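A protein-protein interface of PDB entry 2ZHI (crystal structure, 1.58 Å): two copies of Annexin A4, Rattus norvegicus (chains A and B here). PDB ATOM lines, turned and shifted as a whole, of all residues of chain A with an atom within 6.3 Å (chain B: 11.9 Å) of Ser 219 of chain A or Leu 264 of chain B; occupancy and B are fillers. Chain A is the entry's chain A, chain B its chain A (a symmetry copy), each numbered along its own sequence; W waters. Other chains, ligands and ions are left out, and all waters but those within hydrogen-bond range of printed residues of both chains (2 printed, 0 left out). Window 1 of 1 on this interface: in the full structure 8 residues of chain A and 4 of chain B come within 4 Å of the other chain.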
ATOM      1  N   LEU A 181     -23.079  35.872  16.074  1.00  0.00           N
ATOM      2  CA  LEU A 181     -23.924  36.723  16.933  1.00  0.00           C
ATOM      3  C   LEU A 181     -24.032  36.129  18.330  1.00  0.00           C
ATOM      4  O   LEU A 181     -24.215  36.831  19.324  1.00  0.00           O
ATOM      5  CB  LEU A 181     -25.315  36.922  16.330  1.00  0.00           C
ATOM      6  CG  LEU A 181     -25.363  37.943  15.186  1.00  0.00           C
ATOM      7  CD1 LEU A 181     -26.680  37.840  14.433  1.00  0.00           C
ATOM      8  CD2 LEU A 181     -25.122  39.351  15.708  1.00  0.00           C
ATOM      9  N   TYR A 182     -23.934  34.812  18.395  1.00  0.00           N
ATOM     10  CA  TYR A 182     -23.938  34.102  19.673  1.00  0.00           C
ATOM     11  C   TYR A 182     -22.725  34.443  20.540  1.00  0.00           C
ATOM     12  O   TYR A 182     -22.888  34.816  21.697  1.00  0.00           O
ATOM     13  CB  TYR A 182     -23.991  32.599  19.420  1.00  0.00           C
ATOM     14  CG  TYR A 182     -23.864  31.669  20.606  1.00  0.00           C
ATOM     15  CD1 TYR A 182     -24.988  31.223  21.277  1.00  0.00           C
ATOM     16  CD2 TYR A 182     -22.623  31.209  21.047  1.00  0.00           C
ATOM     17  CE1 TYR A 182     -24.882  30.362  22.359  1.00  0.00           C
ATOM     18  CE2 TYR A 182     -22.505  30.365  22.121  1.00  0.00           C
ATOM     19  CZ  TYR A 182     -23.643  29.946  22.769  1.00  0.00           C
ATOM     20  OH  TYR A 182     -23.502  29.096  23.843  1.00  0.00           O
ATOM     21  N   GLU A 183     -21.511  34.250  20.022  1.00  0.00           N
ATOM     22  CA  GLU A 183     -20.314  34.486  20.835  1.00  0.00           C
ATOM     23  C   GLU A 183     -20.271  35.919  21.349  1.00  0.00           C
ATOM     24  O   GLU A 183     -19.729  36.186  22.422  1.00  0.00           O
ATOM     25  CB  GLU A 183     -19.039  34.183  20.040  1.00  0.00           C
ATOM     26  CG  GLU A 183     -19.031  32.734  19.568  1.00  0.00           C
ATOM     27  CD  GLU A 183     -18.037  32.459  18.462  1.00  0.00           C
ATOM     28  OE1 GLU A 183     -17.984  31.293  18.020  1.00  0.00           O
ATOM     29  OE2 GLU A 183     -17.313  33.385  18.041  1.00  0.00           O
ATOM     30  N   ALA A 184     -20.851  36.804  20.548  1.00  0.00           N
ATOM     31  CA  ALA A 184     -20.964  38.223  20.859  1.00  0.00           C
ATOM     32  C   ALA A 184     -21.900  38.479  22.031  1.00  0.00           C
ATOM     33  O   ALA A 184     -21.847  39.524  22.676  1.00  0.00           O
ATOM     34  CB  ALA A 184     -21.465  39.004  19.643  1.00  0.00           C
ATOM     35  N   GLY A 185     -22.781  37.522  22.308  1.00  0.00           N
ATOM     36  CA  GLY A 185     -23.766  37.690  23.348  1.00  0.00           C
ATOM     37  C   GLY A 185     -23.229  37.120  24.650  1.00  0.00           C
ATOM     38  O   GLY A 185     -23.882  37.155  25.692  1.00  0.00           O
ATOM     39  N   GLU A 186     -22.018  36.573  24.570  1.00  0.00           N
ATOM     40  CA  GLU A 186     -21.476  35.867  25.730  1.00  0.00           C
ATOM     41  C   GLU A 186     -21.156  36.795  26.889  1.00  0.00           C
ATOM     42  O   GLU A 186     -21.508  36.480  28.037  1.00  0.00           O
ATOM     43  CB  GLU A 186     -20.252  35.055  25.264  1.00  0.00           C
ATOM     44  CG  GLU A 186     -20.669  33.846  24.435  1.00  0.00           C
ATOM     45  CD  GLU A 186     -19.561  32.899  24.038  1.00  0.00           C
ATOM     46  OE1 GLU A 186     -18.752  32.475  24.892  1.00  0.00           O
ATOM     47  OE2 GLU A 186     -19.495  32.565  22.833  1.00  0.00           O
ATOM     48  N   GLU A 214     -31.484  29.745  12.747  1.00  0.00           N
ATOM     49  CA  GLU A 214     -30.257  29.150  13.295  1.00  0.00           C
ATOM     50  C   GLU A 214     -29.835  29.811  14.599  1.00  0.00           C
ATOM     51  O   GLU A 214     -29.406  29.170  15.564  1.00  0.00           O
ATOM     52  CB  GLU A 214     -29.132  29.232  12.268  1.00  0.00           C
ATOM     53  CG  GLU A 214     -27.811  28.661  12.751  1.00  0.00           C
ATOM     54  CD  GLU A 214     -27.728  27.154  12.838  1.00  0.00           C
ATOM     55  OE1 GLU A 214     -28.692  26.414  12.540  1.00  0.00           O
ATOM     56  OE2 GLU A 214     -26.625  26.702  13.228  1.00  0.00           O
ATOM     57  N   TYR A 215     -29.954  31.132  14.679  1.00  0.00           N
ATOM     58  CA  TYR A 215     -29.634  31.811  15.925  1.00  0.00           C
ATOM     59  C   TYR A 215     -30.486  31.266  17.071  1.00  0.00           C
ATOM     60  O   TYR A 215     -29.960  31.051  18.167  1.00  0.00           O
ATOM     61  CB  TYR A 215     -29.839  33.338  15.807  1.00  0.00           C
ATOM     62  CG  TYR A 215     -29.416  34.017  17.089  1.00  0.00           C
ATOM     63  CD1 TYR A 215     -30.371  34.419  18.019  1.00  0.00           C
ATOM     64  CD2 TYR A 215     -28.084  34.233  17.401  1.00  0.00           C
ATOM     65  CE1 TYR A 215     -30.007  35.032  19.206  1.00  0.00           C
ATOM     66  CE2 TYR A 215     -27.704  34.842  18.579  1.00  0.00           C
ATOM     67  CZ  TYR A 215     -28.672  35.235  19.477  1.00  0.00           C
ATOM     68  OH  TYR A 215     -28.310  35.848  20.660  1.00  0.00           O
ATOM     69  N   LYS A 216     -31.783  31.068  16.825  1.00  0.00           N
ATOM     70  CA  LYS A 216     -32.658  30.560  17.891  1.00  0.00           C
ATOM     71  C   LYS A 216     -32.190  29.172  18.313  1.00  0.00           C
ATOM     72  O   LYS A 216     -32.153  28.866  19.512  1.00  0.00           O
ATOM     73  CB  LYS A 216     -34.118  30.523  17.457  1.00  0.00           C
ATOM     74  CG  LYS A 216     -35.112  29.929  18.448  1.00  0.00           C
ATOM     75  CD  LYS A 216     -35.125  30.724  19.739  1.00  0.00           C
ATOM     76  CE  LYS A 216     -36.367  30.466  20.581  1.00  0.00           C
ATOM     77  NZ  LYS A 216     -36.565  28.999  20.777  1.00  0.00           N
ATOM     78  N   ARG A 217     -31.852  28.361  17.319  1.00  0.00           N
ATOM     79  CA  ARG A 217     -31.388  27.002  17.570  1.00  0.00           C
ATOM     80  C   ARG A 217     -30.132  26.969  18.430  1.00  0.00           C
ATOM     81  O   ARG A 217     -30.052  26.182  19.387  1.00  0.00           O
ATOM     82  CB  ARG A 217     -31.089  26.275  16.250  1.00  0.00           C
ATOM     83  CG  ARG A 217     -30.822  24.786  16.448  1.00  0.00           C
ATOM     84  CD  ARG A 217     -30.239  24.117  15.221  1.00  0.00           C
ATOM     85  NE  ARG A 217     -28.913  24.558  14.850  1.00  0.00           N
ATOM     86  CZ  ARG A 217     -27.731  24.086  15.220  1.00  0.00           C
ATOM     87  NH1 ARG A 217     -27.648  23.060  16.059  1.00  0.00           N
ATOM     88  NH2 ARG A 217     -26.614  24.648  14.750  1.00  0.00           N
ATOM     89  N   ILE A 218     -29.134  27.807  18.106  1.00  0.00           N
ATOM     90  CA  ILE A 218     -27.899  27.663  18.902  1.00  0.00           C
ATOM     91  C   ILE A 218     -27.914  28.451  20.199  1.00  0.00           C
ATOM     92  O   ILE A 218     -27.145  28.076  21.101  1.00  0.00           O
ATOM     93  CB  ILE A 218     -26.662  28.045  18.065  1.00  0.00           C
ATOM     94  CG1 ILE A 218     -26.513  29.519  17.700  1.00  0.00           C
ATOM     95  CG2 ILE A 218     -26.653  27.201  16.793  1.00  0.00           C
ATOM     96  CD1 ILE A 218     -25.236  29.773  16.914  1.00  0.00           C
ATOM     97  N   SER A 219     -28.710  29.488  20.356  1.00  0.00           N
ATOM     98  CA  SER A 219     -28.687  30.293  21.573  1.00  0.00           C
ATOM     99  C   SER A 219     -29.900  30.046  22.484  1.00  0.00           C
ATOM    100  O   SER A 219     -29.798  30.453  23.655  1.00  0.00           O
ATOM    101  CB  SER A 219     -28.682  31.794  21.292  1.00  0.00           C
ATOM    102  OG  SER A 219     -29.990  32.109  20.794  1.00  0.00           O
ATOM    103  N   GLN A 220     -30.939  29.446  21.933  1.00  0.00           N
ATOM    104  CA  GLN A 220     -32.210  29.221  22.608  1.00  0.00           C
ATOM    105  C   GLN A 220     -32.959  30.529  22.818  1.00  0.00           C
ATOM    106  O   GLN A 220     -33.975  30.594  23.516  1.00  0.00           O
ATOM    107  CB  GLN A 220     -32.004  28.509  23.951  1.00  0.00           C
ATOM    108  CG  GLN A 220     -31.402  27.117  23.775  1.00  0.00           C
ATOM    109  CD  GLN A 220     -32.296  26.192  22.986  1.00  0.00           C
ATOM    110  OE1 GLN A 220     -31.988  25.791  21.858  1.00  0.00           O
ATOM    111  NE2 GLN A 220     -33.426  25.818  23.584  1.00  0.00           N
ATOM    112  N   LYS A 221     -32.463  31.590  22.191  1.00  0.00           N
ATOM    113  CA  LYS A 221     -33.107  32.889  22.285  1.00  0.00           C
ATOM    114  C   LYS A 221     -33.529  33.370  20.897  1.00  0.00           C
ATOM    115  O   LYS A 221     -32.808  33.100  19.952  1.00  0.00           O
ATOM    116  CB  LYS A 221     -32.181  33.937  22.899  1.00  0.00           C
ATOM    117  CG  LYS A 221     -31.846  33.685  24.365  1.00  0.00           C
ATOM    118  CD  LYS A 221     -32.719  34.568  25.254  1.00  0.00           C
ATOM    119  CE  LYS A 221     -32.616  34.182  26.721  1.00  0.00           C
ATOM    120  NZ  LYS A 221     -33.958  33.876  27.303  1.00  0.00           N
ATOM    121  N   ASP A 222     -34.660  34.074  20.816  1.00  0.00           N
ATOM    122  CA  ASP A 222     -34.976  34.769  19.563  1.00  0.00           C
ATOM    123  C   ASP A 222     -33.991  35.921  19.375  1.00  0.00           C
ATOM    124  O   ASP A 222     -33.626  36.545  20.382  1.00  0.00           O
ATOM    125  CB  ASP A 222     -36.408  35.298  19.575  1.00  0.00           C
ATOM    126  CG  ASP A 222     -36.906  35.698  18.193  1.00  0.00           C
ATOM    127  OD1 ASP A 222     -37.293  34.807  17.402  1.00  0.00           O
ATOM    128  OD2 ASP A 222     -36.913  36.913  17.900  1.00  0.00           O
ATOM    129  N   ILE A 223     -33.583  36.204  18.149  1.00  0.00           N
ATOM    130  CA  ILE A 223     -32.650  37.303  17.881  1.00  0.00           C
ATOM    131  C   ILE A 223     -33.142  38.617  18.463  1.00  0.00           C
ATOM    132  O   ILE A 223     -32.364  39.473  18.921  1.00  0.00           O
ATOM    133  CB  ILE A 223     -32.384  37.451  16.369  1.00  0.00           C
ATOM    134  CG1 ILE A 223     -31.166  38.324  16.024  1.00  0.00           C
ATOM    135  CG2 ILE A 223     -33.614  37.940  15.614  1.00  0.00           C
ATOM    136  CD1 ILE A 223     -30.612  37.989  14.657  1.00  0.00           C
ATOM    137  N   SER A 226     -32.091  39.020  22.165  1.00  0.00           N
ATOM    138  CA  SER A 226     -30.701  39.403  22.367  1.00  0.00           C
ATOM    139  C   SER A 226     -30.454  40.847  21.919  1.00  0.00           C
ATOM    140  O   SER A 226     -29.679  41.562  22.560  1.00  0.00           O
ATOM    141  CB  SER A 226     -29.746  38.454  21.657  1.00  0.00           C
ATOM    142  OG  SER A 226     -29.945  37.098  22.082  1.00  0.00           O
ATOM    143  N   GLU A 230     -28.752  43.416  24.424  1.00  0.00           N
ATOM    144  CA  GLU A 230     -27.362  43.726  24.085  1.00  0.00           C
ATOM    145  C   GLU A 230     -27.114  45.115  23.533  1.00  0.00           C
ATOM    146  O   GLU A 230     -25.971  45.596  23.536  1.00  0.00           O
ATOM    147  CB  GLU A 230     -26.889  42.688  23.055  1.00  0.00           C
ATOM    148  CG  GLU A 230     -26.682  41.313  23.688  1.00  0.00           C
ATOM    149  CD  GLU A 230     -26.440  40.248  22.630  1.00  0.00           C
ATOM    150  OE1 GLU A 230     -26.705  39.061  22.910  1.00  0.00           O
ATOM    151  OE2 GLU A 230     -25.984  40.615  21.523  1.00  0.00           O
ATOM    152  N   ARG B 256     -35.610  21.101  33.491  1.00  0.00           N
ATOM    153  CA  ARG B 256     -35.043  22.249  34.170  1.00  0.00           C
ATOM    154  C   ARG B 256     -33.531  22.330  33.989  1.00  0.00           C
ATOM    155  O   ARG B 256     -32.959  23.387  33.766  1.00  0.00           O
ATOM    156  CB  ARG B 256     -35.348  22.212  35.683  1.00  0.00           C
ATOM    157  CG  ARG B 256     -36.779  22.617  36.034  1.00  0.00           C
ATOM    158  CD  ARG B 256     -36.952  24.124  35.843  1.00  0.00           C
ATOM    159  NE  ARG B 256     -36.544  24.984  36.962  1.00  0.00           N
ATOM    160  CZ  ARG B 256     -36.488  26.307  36.877  1.00  0.00           C
ATOM    161  NH1 ARG B 256     -36.794  26.927  35.729  1.00  0.00           N
ATOM    162  NH2 ARG B 256     -36.123  27.101  37.876  1.00  0.00           N
ATOM    163  N   LEU B 257     -32.841  21.209  34.101  1.00  0.00           N
ATOM    164  CA  LEU B 257     -31.401  21.137  33.951  1.00  0.00           C
ATOM    165  C   LEU B 257     -30.973  21.504  32.515  1.00  0.00           C
ATOM    166  O   LEU B 257     -30.071  22.308  32.301  1.00  0.00           O
ATOM    167  CB  LEU B 257     -30.949  19.704  34.287  1.00  0.00           C
ATOM    168  CG  LEU B 257     -30.930  19.404  35.799  1.00  0.00           C
ATOM    169  CD1 LEU B 257     -30.900  17.910  36.085  1.00  0.00           C
ATOM    170  CD2 LEU B 257     -29.734  20.079  36.457  1.00  0.00           C
ATOM    171  N   TYR B 258     -31.694  20.882  31.579  1.00  0.00           N
ATOM    172  CA  TYR B 258     -31.407  21.210  30.170  1.00  0.00           C
ATOM    173  C   TYR B 258     -31.498  22.695  29.895  1.00  0.00           C
ATOM    174  O   TYR B 258     -30.609  23.315  29.303  1.00  0.00           O
ATOM    175  CB  TYR B 258     -32.423  20.495  29.289  1.00  0.00           C
ATOM    176  CG  TYR B 258     -32.275  20.708  27.793  1.00  0.00           C
ATOM    177  CD1 TYR B 258     -31.396  19.939  27.051  1.00  0.00           C
ATOM    178  CD2 TYR B 258     -33.067  21.673  27.178  1.00  0.00           C
ATOM    179  CE1 TYR B 258     -31.300  20.164  25.674  1.00  0.00           C
ATOM    180  CE2 TYR B 258     -32.967  21.883  25.812  1.00  0.00           C
ATOM    181  CZ  TYR B 258     -32.081  21.122  25.087  1.00  0.00           C
ATOM    182  OH  TYR B 258     -31.994  21.341  23.719  1.00  0.00           O
ATOM    183  N   LYS B 259     -32.625  23.275  30.335  1.00  0.00           N
ATOM    184  CA  LYS B 259     -32.836  24.690  30.013  1.00  0.00           C
ATOM    185  C   LYS B 259     -31.873  25.563  30.785  1.00  0.00           C
ATOM    186  O   LYS B 259     -31.564  26.688  30.376  1.00  0.00           O
ATOM    187  CB  LYS B 259     -34.307  25.073  30.255  1.00  0.00           C
ATOM    188  CG  LYS B 259     -35.243  24.397  29.254  1.00  0.00           C
ATOM    189  CD  LYS B 259     -36.702  24.723  29.502  1.00  0.00           C
ATOM    190  CE  LYS B 259     -37.632  23.892  28.626  1.00  0.00           C
ATOM    191  NZ  LYS B 259     -38.668  24.709  27.934  1.00  0.00           N
ATOM    192  N   SER B 260     -31.323  25.097  31.909  1.00  0.00           N
ATOM    193  CA  SER B 260     -30.365  25.919  32.634  1.00  0.00           C
ATOM    194  C   SER B 260     -29.003  25.951  31.939  1.00  0.00           C
ATOM    195  O   SER B 260     -28.195  26.829  32.221  1.00  0.00           O
ATOM    196  CB  SER B 260     -30.159  25.425  34.062  1.00  0.00           C
ATOM    197  OG  SER B 260     -29.311  24.268  34.143  1.00  0.00           O
ATOM    198  N   MET B 261     -28.738  25.004  31.040  1.00  0.00           N
ATOM    199  CA  MET B 261     -27.422  24.928  30.418  1.00  0.00           C
ATOM    200  C   MET B 261     -27.404  25.174  28.917  1.00  0.00           C
ATOM    201  O   MET B 261     -26.422  25.698  28.379  1.00  0.00           O
ATOM    202  CB  MET B 261     -26.856  23.506  30.695  1.00  0.00           C
ATOM    203  CG  MET B 261     -26.357  23.395  32.133  1.00  0.00           C
ATOM    204  SD  MET B 261     -25.659  21.774  32.529  1.00  0.00           S
ATOM    205  CE  MET B 261     -27.151  20.800  32.647  1.00  0.00           C
ATOM    206  N   LYS B 262     -28.442  24.737  28.220  1.00  0.00           N
ATOM    207  CA  LYS B 262     -28.485  24.772  26.763  1.00  0.00           C
ATOM    208  C   LYS B 262     -28.589  26.207  26.264  1.00  0.00           C
ATOM    209  O   LYS B 262     -29.338  27.022  26.805  1.00  0.00           O
ATOM    210  CB  LYS B 262     -29.677  23.959  26.254  1.00  0.00           C
ATOM    211  CG  LYS B 262     -29.809  23.917  24.738  1.00  0.00           C
ATOM    212  CD  LYS B 262     -28.796  22.951  24.112  1.00  0.00           C
ATOM    213  CE  LYS B 262     -29.231  22.662  22.673  1.00  0.00           C
ATOM    214  NZ  LYS B 262     -28.295  21.769  21.932  1.00  0.00           N
ATOM    215  N   GLY B 263     -27.820  26.468  25.205  1.00  0.00           N
ATOM    216  CA  GLY B 263     -27.915  27.806  24.621  1.00  0.00           C
ATOM    217  C   GLY B 263     -27.002  28.774  25.343  1.00  0.00           C
ATOM    218  O   GLY B 263     -26.154  28.399  26.139  1.00  0.00           O
ATOM    219  N   LEU B 264     -27.201  30.045  25.035  1.00  0.00           N
ATOM    220  CA  LEU B 264     -26.444  31.178  25.505  1.00  0.00           C
ATOM    221  C   LEU B 264     -26.665  31.396  27.002  1.00  0.00           C
ATOM    222  O   LEU B 264     -27.795  31.624  27.433  1.00  0.00           O
ATOM    223  CB  LEU B 264     -26.850  32.409  24.698  1.00  0.00           C
ATOM    224  CG  LEU B 264     -26.010  33.668  24.854  1.00  0.00           C
ATOM    225  CD1 LEU B 264     -24.538  33.380  24.621  1.00  0.00           C
ATOM    226  CD2 LEU B 264     -26.530  34.727  23.885  1.00  0.00           C
ATOM    227  N   GLY B 265     -25.543  31.306  27.707  1.00  0.00           N
ATOM    228  CA  GLY B 265     -25.471  31.518  29.127  1.00  0.00           C
ATOM    229  C   GLY B 265     -25.809  30.275  29.935  1.00  0.00           C
ATOM    230  O   GLY B 265     -26.222  29.257  29.366  1.00  0.00           O
ATOM    231  N   THR B 266     -25.617  30.408  31.247  1.00  0.00           N
ATOM    232  CA  THR B 266     -25.908  29.347  32.192  1.00  0.00           C
ATOM    233  C   THR B 266     -26.634  29.906  33.415  1.00  0.00           C
ATOM    234  O   THR B 266     -26.216  30.919  33.979  1.00  0.00           O
ATOM    235  CB  THR B 266     -24.638  28.634  32.658  1.00  0.00           C
ATOM    236  OG1 THR B 266     -24.084  27.973  31.499  1.00  0.00           O
ATOM    237  CG2 THR B 266     -24.924  27.540  33.674  1.00  0.00           C
ATOM    238  N   ASP B 267     -27.705  29.204  33.767  1.00  0.00           N
ATOM    239  CA  ASP B 267     -28.467  29.590  34.962  1.00  0.00           C
ATOM    240  C   ASP B 267     -27.905  28.739  36.105  1.00  0.00           C
ATOM    241  O   ASP B 267     -28.471  27.690  36.410  1.00  0.00           O
ATOM    242  CB  ASP B 267     -29.958  29.387  34.787  1.00  0.00           C
ATOM    243  CG  ASP B 267     -30.812  29.724  35.985  1.00  0.00           C
ATOM    244  OD1 ASP B 267     -30.218  30.202  36.969  1.00  0.00           O
ATOM    245  OD2 ASP B 267     -32.052  29.509  35.935  1.00  0.00           O
ATOM    246  N   ASP B 268     -26.802  29.167  36.693  1.00  0.00           N
ATOM    247  CA  ASP B 268     -26.146  28.290  37.663  1.00  0.00           C
ATOM    248  C   ASP B 268     -27.026  28.118  38.886  1.00  0.00           C
ATOM    249  O   ASP B 268     -26.980  27.085  39.537  1.00  0.00           O
ATOM    250  CB  ASP B 268     -24.796  28.844  38.116  1.00  0.00           C
ATOM    251  CG  ASP B 268     -23.814  28.884  36.952  1.00  0.00           C
ATOM    252  OD1 ASP B 268     -23.319  27.817  36.555  1.00  0.00           O
ATOM    253  OD2 ASP B 268     -23.562  30.000  36.469  1.00  0.00           O
ATOM    254  N   PHE B 301     -23.360  17.273  29.710  1.00  0.00           N
ATOM    255  CA  PHE B 301     -23.809  18.662  29.732  1.00  0.00           C
ATOM    256  C   PHE B 301     -23.096  19.421  30.853  1.00  0.00           C
ATOM    257  O   PHE B 301     -22.583  20.512  30.628  1.00  0.00           O
ATOM    258  CB  PHE B 301     -25.315  18.780  29.947  1.00  0.00           C
ATOM    259  CG  PHE B 301     -26.168  19.020  28.724  1.00  0.00           C
ATOM    260  CD1 PHE B 301     -26.242  18.060  27.728  1.00  0.00           C
ATOM    261  CD2 PHE B 301     -26.878  20.206  28.606  1.00  0.00           C
ATOM    262  CE1 PHE B 301     -27.027  18.284  26.609  1.00  0.00           C
ATOM    263  CE2 PHE B 301     -27.659  20.436  27.485  1.00  0.00           C
ATOM    264  CZ  PHE B 301     -27.730  19.474  26.498  1.00  0.00           C
ATOM    265  N   GLY B 304     -19.504  19.882  29.955  1.00  0.00           N
ATOM    266  CA  GLY B 304     -19.229  20.876  28.917  1.00  0.00           C
ATOM    267  C   GLY B 304     -19.647  22.285  29.232  1.00  0.00           C
ATOM    268  O   GLY B 304     -19.315  23.226  28.490  1.00  0.00           O
ATOM    269  N   ASP B 305     -20.377  22.532  30.332  1.00  0.00           N
ATOM    270  CA  ASP B 305     -20.884  23.850  30.605  1.00  0.00           C
ATOM    271  C   ASP B 305     -20.399  24.463  31.930  1.00  0.00           C
ATOM    272  O   ASP B 305     -20.792  25.599  32.208  1.00  0.00           O
ATOM    273  CB  ASP B 305     -22.419  23.803  30.625  1.00  0.00           C
ATOM    274  CG  ASP B 305     -23.033  25.164  30.389  1.00  0.00           C
ATOM    275  OD1 ASP B 305     -22.661  25.844  29.417  1.00  0.00           O
ATOM    276  OD2 ASP B 305     -23.914  25.575  31.189  1.00  0.00           O
ATOM    277  N   THR B 306     -19.592  23.760  32.717  1.00  0.00           N
ATOM    278  CA  THR B 306     -19.041  24.266  33.975  1.00  0.00           C
ATOM    279  C   THR B 306     -17.571  23.911  34.088  1.00  0.00           C
ATOM    280  O   THR B 306     -17.095  23.097  33.285  1.00  0.00           O
ATOM    281  CB  THR B 306     -19.766  23.665  35.209  1.00  0.00           C
ATOM    282  OG1 THR B 306     -19.512  22.255  35.224  1.00  0.00           O
ATOM    283  CG2 THR B 306     -21.254  23.926  35.094  1.00  0.00           C
HETATM  284  O   HOH W   1     -30.216  30.936  26.424  1.00  0.00           O
HETATM  285  O   HOH W   2     -34.012  22.965  22.509  1.00  0.00           O
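The backbone carbonyl oxygen of Ser 219 of chain A sits at hydrogen-bond distance from the backbone NH of Leu 264 of chain B, 3.0 Å away.
The side-chain amide oxygen (OE1) of Gln 220 of chain A lies close to the backbone carbonyl oxygen (O) of Arg 217 of chain A.
The side-chain hydroxyl (OG) of Ser 219 of chain A lies within hydrogen-bond range of the backbone NH (N) of Lys 221 of chain A (2.9 Å).
OG of Ser 219 of chain A sits at hydrogen-bond distance from O of Tyr 215 of chain A, at 2.8 Å.
The side-chain hydroxyl (OG) of Ser 226 of chain A sits at hydrogen-bond distance from the side-chain hydroxyl (OH) of Tyr 215 of chain A, at 2.5 Å.
Among the printed residues, merely in contact across the chains: Ser 219 of chain A with Gly 263 of chain B (3.4 Å), Tyr 182 of chain A with Leu 264 of chain B (3.6 Å), Tyr 182 of chain A with Gly 263 of chain B (3.6 Å), Ile 218 of chain A with Gly 263 of chain B (3.6 Å), Gln 220 of chain A with Gly 263 of chain B (3.7 Å), Gln 220 of chain A with Lys 262 of chain B (3.7 Å), Tyr 215 of chain A with Leu 264 of chain B (3.9 Å), Glu 186 of chain A with Leu 264 of chain B (3.9 Å) and Gly 185 of chain A with Leu 264 of chain B (3.96 Å).
Ser 219 of chain A touches just these residues of chain B: Gly 263 and Leu 264.
Leu 264 of chain B touches just these residues of chain A: Tyr 182, Gly 185, Glu 186, Tyr 215 and Ser 219.
Of the printed residues of chain B, Gly 185 of chain A touches Leu 264 (3.96 Å).
Glu 186 of chain A touches one residue of chain B.
Of chain B, only Leu 264 comes within 4 Å of Tyr 215 of chain A.
No residue of chain B comes within 4 Å of Lys 216 of chain A.
Arg 217 of chain A touches none of the printed residues of chain B.
Of the printed residues of chain B, Ile 218 of chain A touches Gly 263 (3.6 Å).
Of the printed residues of chain B, Gln 220 of chain A touches Lys 262 and Gly 263.
Printed residues of chain A within 4 Å of Gly 263 of chain B: Tyr 182, Ile 218, Ser 219 and Gln 220.
Of the printed residues of chain A, Lys 262 of chain B touches Gln 220 (3.7 Å).
The nearest residue of chain B that does not touch Ser 219 of chain A is Lys 262 of chain B (4.7 Å).
The nearest residue of chain A that does not touch Leu 264 of chain B is Ile 218 of chain A (4.4 Å).
Of the 18 printed residues of chain A, 7 touch a printed residue of chain B.
Printed residues of chain A that touch a printed residue of chain B: Tyr 182, Gly 185, Glu 186, Tyr 215, Ile 218, Ser 219 and Gln 220.
Hydrophobic or aromatic side chains of chain A within 4 Å of the printed part of chain B: Tyr 182 and Tyr 215.
Hydrophobic or aromatic side chains of chain B that line the printed part of chain A: Leu 264.
Along chain B the printed residues that touch a printed residue of chain A span positions 262 to 264.
Among the printed residues, no Asp or Glu carboxylate lies within 4 Å of a Lys or Arg side-chain nitrogen of the other chain.
No position is printed for both chains.
Water W1 lies within hydrogen-bond range of O of Leu 264 of chain B (2.7 Å) and O of Ser 219 of chain A (2.8 Å).
Water W2 lies within hydrogen-bond range of the side-chain hydroxyl (OH) of Tyr 258 of chain B and the side-chain amide nitrogen (NE2) of Gln 220 of chain A.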
